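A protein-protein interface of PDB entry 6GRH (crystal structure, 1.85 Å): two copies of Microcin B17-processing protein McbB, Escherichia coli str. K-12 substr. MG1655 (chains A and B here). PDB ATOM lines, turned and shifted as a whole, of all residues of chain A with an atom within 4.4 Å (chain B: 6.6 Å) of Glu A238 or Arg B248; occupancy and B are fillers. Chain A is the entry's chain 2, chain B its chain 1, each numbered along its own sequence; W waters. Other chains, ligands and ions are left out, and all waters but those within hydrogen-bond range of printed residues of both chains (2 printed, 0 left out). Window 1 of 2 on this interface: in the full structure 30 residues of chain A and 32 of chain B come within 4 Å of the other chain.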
ATOM      1  N   LEU A 234     -17.668 -17.593  -7.782  1.00  0.00           N
ATOM      2  CA  LEU A 234     -18.528 -16.818  -6.859  1.00  0.00           C
ATOM      3  C   LEU A 234     -19.402 -15.832  -7.617  1.00  0.00           C
ATOM      4  O   LEU A 234     -18.935 -15.204  -8.536  1.00  0.00           O
ATOM      5  CB  LEU A 234     -17.695 -16.007  -5.904  1.00  0.00           C
ATOM      6  CG  LEU A 234     -16.848 -16.725  -4.887  1.00  0.00           C
ATOM      7  CD1 LEU A 234     -16.196 -15.670  -3.996  1.00  0.00           C
ATOM      8  CD2 LEU A 234     -17.681 -17.709  -4.108  1.00  0.00           C
ATOM      9  N   GLY A 235     -20.665 -15.715  -7.229  1.00  0.00           N
ATOM     10  CA  GLY A 235     -21.542 -14.664  -7.717  1.00  0.00           C
ATOM     11  C   GLY A 235     -21.977 -13.793  -6.560  1.00  0.00           C
ATOM     12  O   GLY A 235     -21.471 -13.910  -5.431  1.00  0.00           O
ATOM     13  N   GLU A 236     -22.935 -12.933  -6.835  1.00  0.00           N
ATOM     14  CA  GLU A 236     -23.461 -12.021  -5.813  1.00  0.00           C
ATOM     15  C   GLU A 236     -23.987 -12.773  -4.579  1.00  0.00           C
ATOM     16  O   GLU A 236     -23.721 -12.347  -3.447  1.00  0.00           O
ATOM     17  CB  GLU A 236     -24.573 -11.147  -6.369  1.00  0.00           C
ATOM     18  CG  GLU A 236     -25.037 -10.053  -5.410  1.00  0.00           C
ATOM     19  CD  GLU A 236     -26.220  -9.237  -5.949  1.00  0.00           C
ATOM     20  OE1 GLU A 236     -26.257  -8.922  -7.156  1.00  0.00           O
ATOM     21  OE2 GLU A 236     -27.121  -8.900  -5.156  1.00  0.00           O
ATOM     22  N   SER A 237     -24.731 -13.855  -4.785  1.00  0.00           N
ATOM     23  CA  SER A 237     -25.351 -14.535  -3.638  1.00  0.00           C
ATOM     24  C   SER A 237     -24.307 -15.160  -2.698  1.00  0.00           C
ATOM     25  O   SER A 237     -24.434 -15.070  -1.478  1.00  0.00           O
ATOM     26  CB  SER A 237     -26.408 -15.539  -4.074  1.00  0.00           C
ATOM     27  OG  SER A 237     -25.849 -16.693  -4.620  1.00  0.00           O
ATOM     28  N   GLU A 238     -23.265 -15.753  -3.265  1.00  0.00           N
ATOM     29  CA  GLU A 238     -22.230 -16.368  -2.445  1.00  0.00           C
ATOM     30  C   GLU A 238     -21.504 -15.316  -1.633  1.00  0.00           C
ATOM     31  O   GLU A 238     -21.176 -15.563  -0.466  1.00  0.00           O
ATOM     32  CB  GLU A 238     -21.230 -17.139  -3.274  1.00  0.00           C
ATOM     33  CG  GLU A 238     -21.760 -18.447  -3.828  1.00  0.00           C
ATOM     34  CD  GLU A 238     -22.614 -18.294  -5.095  1.00  0.00           C
ATOM     35  OE1 GLU A 238     -22.489 -17.274  -5.815  1.00  0.00           O
ATOM     36  OE2 GLU A 238     -23.447 -19.199  -5.340  1.00  0.00           O
ATOM     37  N   ARG A 239     -21.274 -14.150  -2.235  1.00  0.00           N
ATOM     38  CA  ARG A 239     -20.648 -13.059  -1.546  1.00  0.00           C
ATOM     39  C   ARG A 239     -21.546 -12.479  -0.432  1.00  0.00           C
ATOM     40  O   ARG A 239     -21.041 -12.151   0.638  1.00  0.00           O
ATOM     41  CB  ARG A 239     -20.204 -11.987  -2.536  1.00  0.00           C
ATOM     42  CG  ARG A 239     -19.023 -12.459  -3.396  1.00  0.00           C
ATOM     43  CD  ARG A 239     -18.721 -11.479  -4.506  1.00  0.00           C
ATOM     44  NE  ARG A 239     -17.515 -11.874  -5.204  1.00  0.00           N
ATOM     45  CZ  ARG A 239     -17.396 -12.059  -6.513  1.00  0.00           C
ATOM     46  NH1 ARG A 239     -18.419 -11.844  -7.344  1.00  0.00           N
ATOM     47  NH2 ARG A 239     -16.212 -12.441  -7.009  1.00  0.00           N
ATOM     48  N   GLY A 240     -22.861 -12.371  -0.666  1.00  0.00           N
ATOM     49  CA  GLY A 240     -23.796 -11.919   0.375  1.00  0.00           C
ATOM     50  C   GLY A 240     -23.838 -12.895   1.548  1.00  0.00           C
ATOM     51  O   GLY A 240     -23.870 -12.490   2.689  1.00  0.00           O
ATOM     52  N   PHE A 241     -23.852 -14.190   1.253  1.00  0.00           N
ATOM     53  CA  PHE A 241     -23.777 -15.220   2.262  1.00  0.00           C
ATOM     54  C   PHE A 241     -22.498 -15.076   3.096  1.00  0.00           C
ATOM     55  O   PHE A 241     -22.552 -15.115   4.337  1.00  0.00           O
ATOM     56  CB  PHE A 241     -23.827 -16.568   1.554  1.00  0.00           C
ATOM     57  CG  PHE A 241     -23.888 -17.749   2.458  1.00  0.00           C
ATOM     58  CD1 PHE A 241     -25.082 -18.127   3.062  1.00  0.00           C
ATOM     59  CD2 PHE A 241     -22.789 -18.546   2.624  1.00  0.00           C
ATOM     60  CE1 PHE A 241     -25.153 -19.273   3.854  1.00  0.00           C
ATOM     61  CE2 PHE A 241     -22.853 -19.685   3.412  1.00  0.00           C
ATOM     62  CZ  PHE A 241     -24.026 -20.043   4.038  1.00  0.00           C
ATOM     63  N   SER A 242     -21.353 -14.918   2.410  1.00  0.00           N
ATOM     64  CA  SER A 242     -20.058 -14.736   3.099  1.00  0.00           C
ATOM     65  C   SER A 242     -20.055 -13.478   4.000  1.00  0.00           C
ATOM     66  O   SER A 242     -19.599 -13.521   5.132  1.00  0.00           O
ATOM     67  CB  SER A 242     -18.907 -14.651   2.090  1.00  0.00           C
ATOM     68  OG  SER A 242     -18.846 -15.847   1.331  1.00  0.00           O
ATOM     69  N   LEU A 274     -20.931 -23.838   0.466  1.00  0.00           N
ATOM     70  CA  LEU A 274     -21.662 -22.823  -0.280  1.00  0.00           C
ATOM     71  C   LEU A 274     -22.797 -23.390  -1.122  1.00  0.00           C
ATOM     72  O   LEU A 274     -23.655 -22.634  -1.563  1.00  0.00           O
ATOM     73  CB  LEU A 274     -20.713 -22.051  -1.185  1.00  0.00           C
ATOM     74  CG  LEU A 274     -19.664 -21.199  -0.483  1.00  0.00           C
ATOM     75  CD1 LEU A 274     -18.661 -20.659  -1.498  1.00  0.00           C
ATOM     76  CD2 LEU A 274     -20.318 -20.073   0.276  1.00  0.00           C
ATOM     77  N   ILE A 275     -22.814 -24.702  -1.337  1.00  0.00           N
ATOM     78  CA  ILE A 275     -23.902 -25.332  -2.045  1.00  0.00           C
ATOM     79  C   ILE A 275     -25.074 -25.640  -1.095  1.00  0.00           C
ATOM     80  O   ILE A 275     -26.194 -25.232  -1.353  1.00  0.00           O
ATOM     81  CB  ILE A 275     -23.469 -26.651  -2.711  1.00  0.00           C
ATOM     82  CG1 ILE A 275     -22.281 -26.438  -3.653  1.00  0.00           C
ATOM     83  CG2 ILE A 275     -24.647 -27.241  -3.473  1.00  0.00           C
ATOM     84  CD1 ILE A 275     -21.565 -27.728  -4.007  1.00  0.00           C
ATOM     85  N   CYS A 277     -25.297 -24.771   2.128  1.00  0.00           N
ATOM     86  CA  CYS A 277     -25.395 -23.693   3.107  1.00  0.00           C
ATOM     87  C   CYS A 277     -25.238 -24.205   4.557  1.00  0.00           C
ATOM     88  O   CYS A 277     -25.551 -23.478   5.497  1.00  0.00           O
ATOM     89  CB  CYS A 277     -26.680 -22.886   2.932  1.00  0.00           C
ATOM     90  SG  CYS A 277     -26.872 -22.170   1.254  1.00  0.00           S
ATOM     91  N   PRO B  17     -19.625 -25.186 -11.738  1.00  0.00           N
ATOM     92  CA  PRO B  17     -18.633 -24.198 -11.282  1.00  0.00           C
ATOM     93  C   PRO B  17     -17.186 -24.629 -11.518  1.00  0.00           C
ATOM     94  O   PRO B  17     -16.811 -25.749 -11.166  1.00  0.00           O
ATOM     95  CB  PRO B  17     -18.906 -24.089  -9.769  1.00  0.00           C
ATOM     96  CG  PRO B  17     -20.330 -24.529  -9.625  1.00  0.00           C
ATOM     97  CD  PRO B  17     -20.453 -25.654 -10.622  1.00  0.00           C
ATOM     98  N   TYR B  32     -15.127 -28.439  -8.879  1.00  0.00           N
ATOM     99  CA  TYR B  32     -15.511 -29.112  -7.634  1.00  0.00           C
ATOM    100  C   TYR B  32     -15.053 -30.574  -7.528  1.00  0.00           C
ATOM    101  O   TYR B  32     -14.886 -31.104  -6.424  1.00  0.00           O
ATOM    102  CB  TYR B  32     -17.023 -29.024  -7.476  1.00  0.00           C
ATOM    103  CG  TYR B  32     -17.562 -27.674  -7.059  1.00  0.00           C
ATOM    104  CD1 TYR B  32     -16.732 -26.621  -6.668  1.00  0.00           C
ATOM    105  CD2 TYR B  32     -18.916 -27.469  -6.999  1.00  0.00           C
ATOM    106  CE1 TYR B  32     -17.251 -25.404  -6.262  1.00  0.00           C
ATOM    107  CE2 TYR B  32     -19.443 -26.245  -6.605  1.00  0.00           C
ATOM    108  CZ  TYR B  32     -18.598 -25.228  -6.230  1.00  0.00           C
ATOM    109  OH  TYR B  32     -19.121 -24.037  -5.818  1.00  0.00           O
ATOM    110  N   TRP B 115     -28.990 -15.799 -11.955  1.00  0.00           N
ATOM    111  CA  TRP B 115     -29.285 -17.164 -11.550  1.00  0.00           C
ATOM    112  C   TRP B 115     -29.369 -18.142 -12.706  1.00  0.00           C
ATOM    113  O   TRP B 115     -29.355 -19.338 -12.473  1.00  0.00           O
ATOM    114  CB  TRP B 115     -30.519 -17.231 -10.633  1.00  0.00           C
ATOM    115  CG  TRP B 115     -30.331 -16.491  -9.306  1.00  0.00           C
ATOM    116  CD1 TRP B 115     -29.204 -15.870  -8.850  1.00  0.00           C
ATOM    117  CD2 TRP B 115     -31.326 -16.310  -8.280  1.00  0.00           C
ATOM    118  NE1 TRP B 115     -29.442 -15.304  -7.606  1.00  0.00           N
ATOM    119  CE2 TRP B 115     -30.729 -15.562  -7.234  1.00  0.00           C
ATOM    120  CE3 TRP B 115     -32.669 -16.678  -8.159  1.00  0.00           C
ATOM    121  CZ2 TRP B 115     -31.423 -15.199  -6.066  1.00  0.00           C
ATOM    122  CZ3 TRP B 115     -33.363 -16.308  -6.976  1.00  0.00           C
ATOM    123  CH2 TRP B 115     -32.734 -15.574  -5.972  1.00  0.00           C
ATOM    124  N   ASP B 118     -26.664 -20.627 -12.567  1.00  0.00           N
ATOM    125  CA  ASP B 118     -26.936 -21.755 -11.684  1.00  0.00           C
ATOM    126  C   ASP B 118     -28.024 -22.647 -12.289  1.00  0.00           C
ATOM    127  O   ASP B 118     -28.574 -23.511 -11.601  1.00  0.00           O
ATOM    128  CB  ASP B 118     -27.378 -21.210 -10.314  1.00  0.00           C
ATOM    129  CG  ASP B 118     -26.399 -20.164  -9.757  1.00  0.00           C
ATOM    130  OD1 ASP B 118     -25.312 -20.541  -9.266  1.00  0.00           O
ATOM    131  OD2 ASP B 118     -26.691 -18.947  -9.843  1.00  0.00           O
ATOM    132  N   GLY B 240     -28.816 -10.531   2.067  1.00  0.00           N
ATOM    133  CA  GLY B 240     -27.846 -11.275   1.218  1.00  0.00           C
ATOM    134  C   GLY B 240     -27.828 -12.761   1.506  1.00  0.00           C
ATOM    135  O   GLY B 240     -27.858 -13.589   0.602  1.00  0.00           O
ATOM    136  N   TYR B 243     -31.062 -14.145   0.217  1.00  0.00           N
ATOM    137  CA  TYR B 243     -30.937 -14.209  -1.247  1.00  0.00           C
ATOM    138  C   TYR B 243     -30.220 -15.485  -1.691  1.00  0.00           C
ATOM    139  O   TYR B 243     -30.681 -16.170  -2.601  1.00  0.00           O
ATOM    140  CB  TYR B 243     -30.175 -12.976  -1.718  1.00  0.00           C
ATOM    141  CG  TYR B 243     -30.086 -12.692  -3.192  1.00  0.00           C
ATOM    142  CD1 TYR B 243     -31.183 -12.198  -3.893  1.00  0.00           C
ATOM    143  CD2 TYR B 243     -28.876 -12.834  -3.874  1.00  0.00           C
ATOM    144  CE1 TYR B 243     -31.081 -11.871  -5.247  1.00  0.00           C
ATOM    145  CE2 TYR B 243     -28.763 -12.505  -5.237  1.00  0.00           C
ATOM    146  CZ  TYR B 243     -29.876 -12.012  -5.909  1.00  0.00           C
ATOM    147  OH  TYR B 243     -29.786 -11.707  -7.241  1.00  0.00           O
ATOM    148  N   HIS B 244     -29.109 -15.805  -1.028  1.00  0.00           N
ATOM    149  CA  HIS B 244     -28.395 -17.025  -1.333  1.00  0.00           C
ATOM    150  C   HIS B 244     -29.211 -18.290  -1.041  1.00  0.00           C
ATOM    151  O   HIS B 244     -29.209 -19.231  -1.850  1.00  0.00           O
ATOM    152  CB  HIS B 244     -27.071 -17.047  -0.585  1.00  0.00           C
ATOM    153  CG  HIS B 244     -26.178 -18.168  -0.988  1.00  0.00           C
ATOM    154  ND1 HIS B 244     -25.680 -18.306  -2.273  1.00  0.00           N
ATOM    155  CD2 HIS B 244     -25.706 -19.220  -0.276  1.00  0.00           C
ATOM    156  CE1 HIS B 244     -24.953 -19.410  -2.330  1.00  0.00           C
ATOM    157  NE2 HIS B 244     -24.942 -19.973  -1.131  1.00  0.00           N
ATOM    158  N   LEU B 245     -29.881 -18.335   0.118  1.00  0.00           N
ATOM    159  CA  LEU B 245     -30.738 -19.478   0.442  1.00  0.00           C
ATOM    160  C   LEU B 245     -31.883 -19.712  -0.538  1.00  0.00           C
ATOM    161  O   LEU B 245     -32.176 -20.857  -0.889  1.00  0.00           O
ATOM    162  CB  LEU B 245     -31.267 -19.383   1.878  1.00  0.00           C
ATOM    163  CG  LEU B 245     -30.282 -19.663   2.995  1.00  0.00           C
ATOM    164  CD1 LEU B 245     -30.973 -19.503   4.354  1.00  0.00           C
ATOM    165  CD2 LEU B 245     -29.738 -21.062   2.920  1.00  0.00           C
ATOM    166  N   ILE B 246     -32.499 -18.629  -0.995  1.00  0.00           N
ATOM    167  CA  ILE B 246     -33.528 -18.675  -2.042  1.00  0.00           C
ATOM    168  C   ILE B 246     -32.941 -19.270  -3.330  1.00  0.00           C
ATOM    169  O   ILE B 246     -33.486 -20.238  -3.907  1.00  0.00           O
ATOM    170  CB  ILE B 246     -34.141 -17.285  -2.280  1.00  0.00           C
ATOM    171  CG1 ILE B 246     -34.944 -16.824  -1.051  1.00  0.00           C
ATOM    172  CG2 ILE B 246     -35.066 -17.274  -3.497  1.00  0.00           C
ATOM    173  CD1 ILE B 246     -35.417 -15.387  -1.087  1.00  0.00           C
ATOM    174  N   LYS B 247     -31.806 -18.723  -3.761  1.00  0.00           N
ATOM    175  CA  LYS B 247     -31.142 -19.221  -4.950  1.00  0.00           C
ATOM    176  C   LYS B 247     -30.839 -20.713  -4.872  1.00  0.00           C
ATOM    177  O   LYS B 247     -31.183 -21.480  -5.788  1.00  0.00           O
ATOM    178  CB  LYS B 247     -29.858 -18.438  -5.225  1.00  0.00           C
ATOM    179  CG  LYS B 247     -29.307 -18.777  -6.601  1.00  0.00           C
ATOM    180  CD  LYS B 247     -27.906 -18.251  -6.809  1.00  0.00           C
ATOM    181  CE  LYS B 247     -26.891 -19.234  -6.264  1.00  0.00           C
ATOM    182  NZ  LYS B 247     -25.569 -18.715  -6.626  1.00  0.00           N
ATOM    183  N   ARG B 248     -30.222 -21.133  -3.760  1.00  0.00           N
ATOM    184  CA  ARG B 248     -29.868 -22.526  -3.620  1.00  0.00           C
ATOM    185  C   ARG B 248     -31.062 -23.444  -3.535  1.00  0.00           C
ATOM    186  O   ARG B 248     -31.028 -24.535  -4.079  1.00  0.00           O
ATOM    187  CB  ARG B 248     -28.950 -22.779  -2.440  1.00  0.00           C
ATOM    188  CG  ARG B 248     -27.579 -22.204  -2.650  1.00  0.00           C
ATOM    189  CD  ARG B 248     -26.892 -22.763  -3.902  1.00  0.00           C
ATOM    190  NE  ARG B 248     -25.464 -22.545  -3.794  1.00  0.00           N
ATOM    191  CZ  ARG B 248     -24.604 -22.502  -4.798  1.00  0.00           C
ATOM    192  NH1 ARG B 248     -24.987 -22.678  -6.063  1.00  0.00           N
ATOM    193  NH2 ARG B 248     -23.322 -22.314  -4.516  1.00  0.00           N
ATOM    194  N   ARG B 249     -32.128 -22.978  -2.905  1.00  0.00           N
ATOM    195  CA  ARG B 249     -33.334 -23.759  -2.859  1.00  0.00           C
ATOM    196  C   ARG B 249     -33.979 -23.920  -4.239  1.00  0.00           C
ATOM    197  O   ARG B 249     -34.380 -25.019  -4.624  1.00  0.00           O
ATOM    198  CB  ARG B 249     -34.290 -23.195  -1.781  1.00  0.00           C
ATOM    199  CG  ARG B 249     -35.514 -24.052  -1.573  1.00  0.00           C
ATOM    200  CD  ARG B 249     -35.150 -25.331  -0.847  1.00  0.00           C
ATOM    201  NE  ARG B 249     -36.328 -26.158  -0.670  1.00  0.00           N
ATOM    202  CZ  ARG B 249     -36.467 -27.433  -1.021  1.00  0.00           C
ATOM    203  NH1 ARG B 249     -35.460 -28.147  -1.549  1.00  0.00           N
ATOM    204  NH2 ARG B 249     -37.640 -28.024  -0.797  1.00  0.00           N
ATOM    205  N   LEU B 250     -34.084 -22.844  -4.988  1.00  0.00           N
ATOM    206  CA  LEU B 250     -34.578 -22.923  -6.358  1.00  0.00           C
ATOM    207  C   LEU B 250     -33.708 -23.811  -7.213  1.00  0.00           C
ATOM    208  O   LEU B 250     -34.208 -24.580  -8.052  1.00  0.00           O
ATOM    209  CB  LEU B 250     -34.671 -21.531  -7.005  1.00  0.00           C
ATOM    210  CG  LEU B 250     -35.940 -20.715  -6.788  1.00  0.00           C
ATOM    211  CD1 LEU B 250     -35.741 -19.327  -7.367  1.00  0.00           C
ATOM    212  CD2 LEU B 250     -37.175 -21.397  -7.373  1.00  0.00           C
ATOM    213  N   GLN B 251     -32.393 -23.683  -7.017  1.00  0.00           N
ATOM    214  CA  GLN B 251     -31.429 -24.512  -7.724  1.00  0.00           C
ATOM    215  C   GLN B 251     -31.645 -25.997  -7.440  1.00  0.00           C
ATOM    216  O   GLN B 251     -31.691 -26.793  -8.391  1.00  0.00           O
ATOM    217  CB  GLN B 251     -30.017 -24.059  -7.417  1.00  0.00           C
ATOM    218  CG  GLN B 251     -28.947 -24.823  -8.170  1.00  0.00           C
ATOM    219  CD  GLN B 251     -27.577 -24.195  -8.043  1.00  0.00           C
ATOM    220  OE1 GLN B 251     -27.391 -23.188  -7.349  1.00  0.00           O
ATOM    221  NE2 GLN B 251     -26.630 -24.725  -8.792  1.00  0.00           N
ATOM    222  N   GLU B 252     -31.857 -26.359  -6.161  1.00  0.00           N
ATOM    223  CA  GLU B 252     -32.140 -27.736  -5.796  1.00  0.00           C
ATOM    224  C   GLU B 252     -33.344 -28.291  -6.523  1.00  0.00           C
ATOM    225  O   GLU B 252     -33.329 -29.436  -6.970  1.00  0.00           O
ATOM    226  CB  GLU B 252     -32.445 -27.891  -4.296  1.00  0.00           C
ATOM    227  CG  GLU B 252     -31.261 -27.779  -3.393  1.00  0.00           C
ATOM    228  CD  GLU B 252     -31.647 -27.642  -1.907  1.00  0.00           C
ATOM    229  OE1 GLU B 252     -32.825 -27.853  -1.538  1.00  0.00           O
ATOM    230  OE2 GLU B 252     -30.737 -27.309  -1.114  1.00  0.00           O
ATOM    231  N   LEU B 253     -34.386 -27.478  -6.603  1.00  0.00           N
ATOM    232  CA  LEU B 253     -35.683 -27.898  -7.136  1.00  0.00           C
ATOM    233  C   LEU B 253     -35.764 -27.884  -8.657  1.00  0.00           C
ATOM    234  O   LEU B 253     -36.332 -28.815  -9.230  1.00  0.00           O
ATOM    235  CB  LEU B 253     -36.810 -27.013  -6.579  1.00  0.00           C
ATOM    236  CG  LEU B 253     -37.063 -27.186  -5.064  1.00  0.00           C
ATOM    237  CD1 LEU B 253     -37.885 -26.024  -4.540  1.00  0.00           C
ATOM    238  CD2 LEU B 253     -37.753 -28.498  -4.774  1.00  0.00           C
ATOM    239  N   THR B 256     -29.500 -26.334 -11.850  1.00  0.00           N
ATOM    240  CA  THR B 256     -28.388 -27.263 -12.021  1.00  0.00           C
ATOM    241  C   THR B 256     -28.093 -27.926 -10.674  1.00  0.00           C
ATOM    242  O   THR B 256     -27.596 -27.284  -9.737  1.00  0.00           O
ATOM    243  CB  THR B 256     -27.150 -26.514 -12.539  1.00  0.00           C
ATOM    244  OG1 THR B 256     -27.463 -25.966 -13.817  1.00  0.00           O
ATOM    245  CG2 THR B 256     -25.931 -27.422 -12.623  1.00  0.00           C
ATOM    246  N   LEU B 258     -26.241 -29.715  -7.982  1.00  0.00           N
ATOM    247  CA  LEU B 258     -24.847 -29.952  -7.618  1.00  0.00           C
ATOM    248  C   LEU B 258     -24.678 -31.036  -6.515  1.00  0.00           C
ATOM    249  O   LEU B 258     -23.702 -31.776  -6.510  1.00  0.00           O
ATOM    250  CB  LEU B 258     -24.229 -28.627  -7.164  1.00  0.00           C
ATOM    251  CG  LEU B 258     -24.137 -27.538  -8.232  1.00  0.00           C
ATOM    252  CD1 LEU B 258     -23.641 -26.246  -7.611  1.00  0.00           C
ATOM    253  CD2 LEU B 258     -23.235 -27.990  -9.357  1.00  0.00           C
HETATM  254  O   HOH W   1     -28.363 -26.608  -2.195  1.00  0.00           O
HETATM  255  O   HOH W   2     -26.346 -14.452  -7.284  1.00  0.00           O
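The side-chain hydroxyl (OG) of Ser A237 sits at hydrogen-bond distance from a ring nitrogen (ND1) of His B244.
NE2 of His B244 lies close to SG of Cys A277 (3.8 Å).
The backbone carbonyl oxygen of Leu A274 sits at hydrogen-bond distance from a ring nitrogen (NE2) of His B244 (3.0 Å).
The backbone carbonyl oxygen (O) of Leu A274 sits at hydrogen-bond distance from the guanidinium group (NE) of Arg B248.
OE2 of Glu A238 is in salt-bridge range of NZ of Lys B247, at 2.5 Å.
The guanidinium group (NH2) of Arg B248 lies within salt-bridge range of the side-chain carboxylate (OE2) of Glu A238, 3.2 Å away.
The side-chain amino group of Lys B247 sits at hydrogen-bond distance from the side-chain hydroxyl of Ser A237.
NH1 of Arg B248 is in hydrogen-bond range of OE1 of Gln B251 (2.8 Å).
The side-chain carboxylate of Asp B118 lies within salt-bridge range of the side-chain amino group of Lys B247 (3.2 Å).
The backbone carbonyl oxygen of Glu A238 is in hydrogen-bond range of the side-chain hydroxyl of Ser A242 (3.0 Å).
The side-chain carboxylate (OD1) of Asp B118 lies within salt-bridge range of the guanidinium group (NH1) of Arg B248 (3.9 Å).
N of Gly A235 is in hydrogen-bond range of OE1 of Glu A238 (2.8 Å).
Among the printed residues, pairs that only touch across the chains: Glu A236 with Tyr B243 (3.96 Å), Ser A237 with Tyr B243 (3.7 Å), Glu A238 with His B244 (3.4 Å), Gly A240 with Gly B240 (3.99 Å), Phe A241 with His B244 (3.6 Å), Ile A275 with Tyr B32 (3.7 Å), Ile A275 with Arg B248 (3.6 Å), Ile A275 with Leu B258 (3.96 Å), Cys A277 with Leu B245 (3.5 Å) and Cys A277 with Arg B248 (3.97 Å).
Of chain A, only Glu A238 (3.2 Å), Leu A274 (2.9 Å), Ile A275 (3.6 Å) and Cys A277 (3.97 Å) come within 4 Å of Arg B248.
Of the printed residues of chain B, Gly A240 touches Gly B240 (3.99 Å).
Of the printed residues of chain A, Tyr B32 touches Ile A275 (3.7 Å).
Of the printed residues of chain A, Tyr B243 touches Glu A236 (3.96 Å) and Ser A237 (3.7 Å).
Printed residues of chain B within 4 Å of Phe A241: His B244.
Printed residues of chain A within 4 Å of Gly B240: Gly A240 (3.99 Å).
Arg A239 touches none of the printed residues of chain B.
The nearest printed residue of chain B that does not touch Ile A275 is Glu B252 (5.0 Å).
Of the 18 printed residues of chain B, 8 touch a printed residue of chain A.
Hydrophobic or aromatic side chains of chain B that line the printed part of chain A: Tyr B32, Tyr B243, His B244, Leu B245 and Leu B258.
Along chain B the printed residues that touch a printed residue of chain A span positions 32 to 258.
Printed residues of chain A that touch a printed residue of chain B: Glu A236, Ser A237, Glu A238, Gly A240, Phe A241, Leu A274, Ile A275 and Cys A277.
Hydrophobic or aromatic side chains of chain A that line the printed part of chain B: Phe A241 and Ile A275.
Gly B240 touches its own counterpart, Gly A240.
Position printed for both chains: 240.
Of the 17 pairs that touch across the chains among the printed residues, 1 has its exchanged pair printed and touching as well.
Water W1 lies within hydrogen-bond range of OE2 of Glu B252 and O of Ile A275.
Water W2 lies within hydrogen-bond range of N of Ser A237 (3.0 Å) and NE1 of Trp B115 (3.2 Å).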
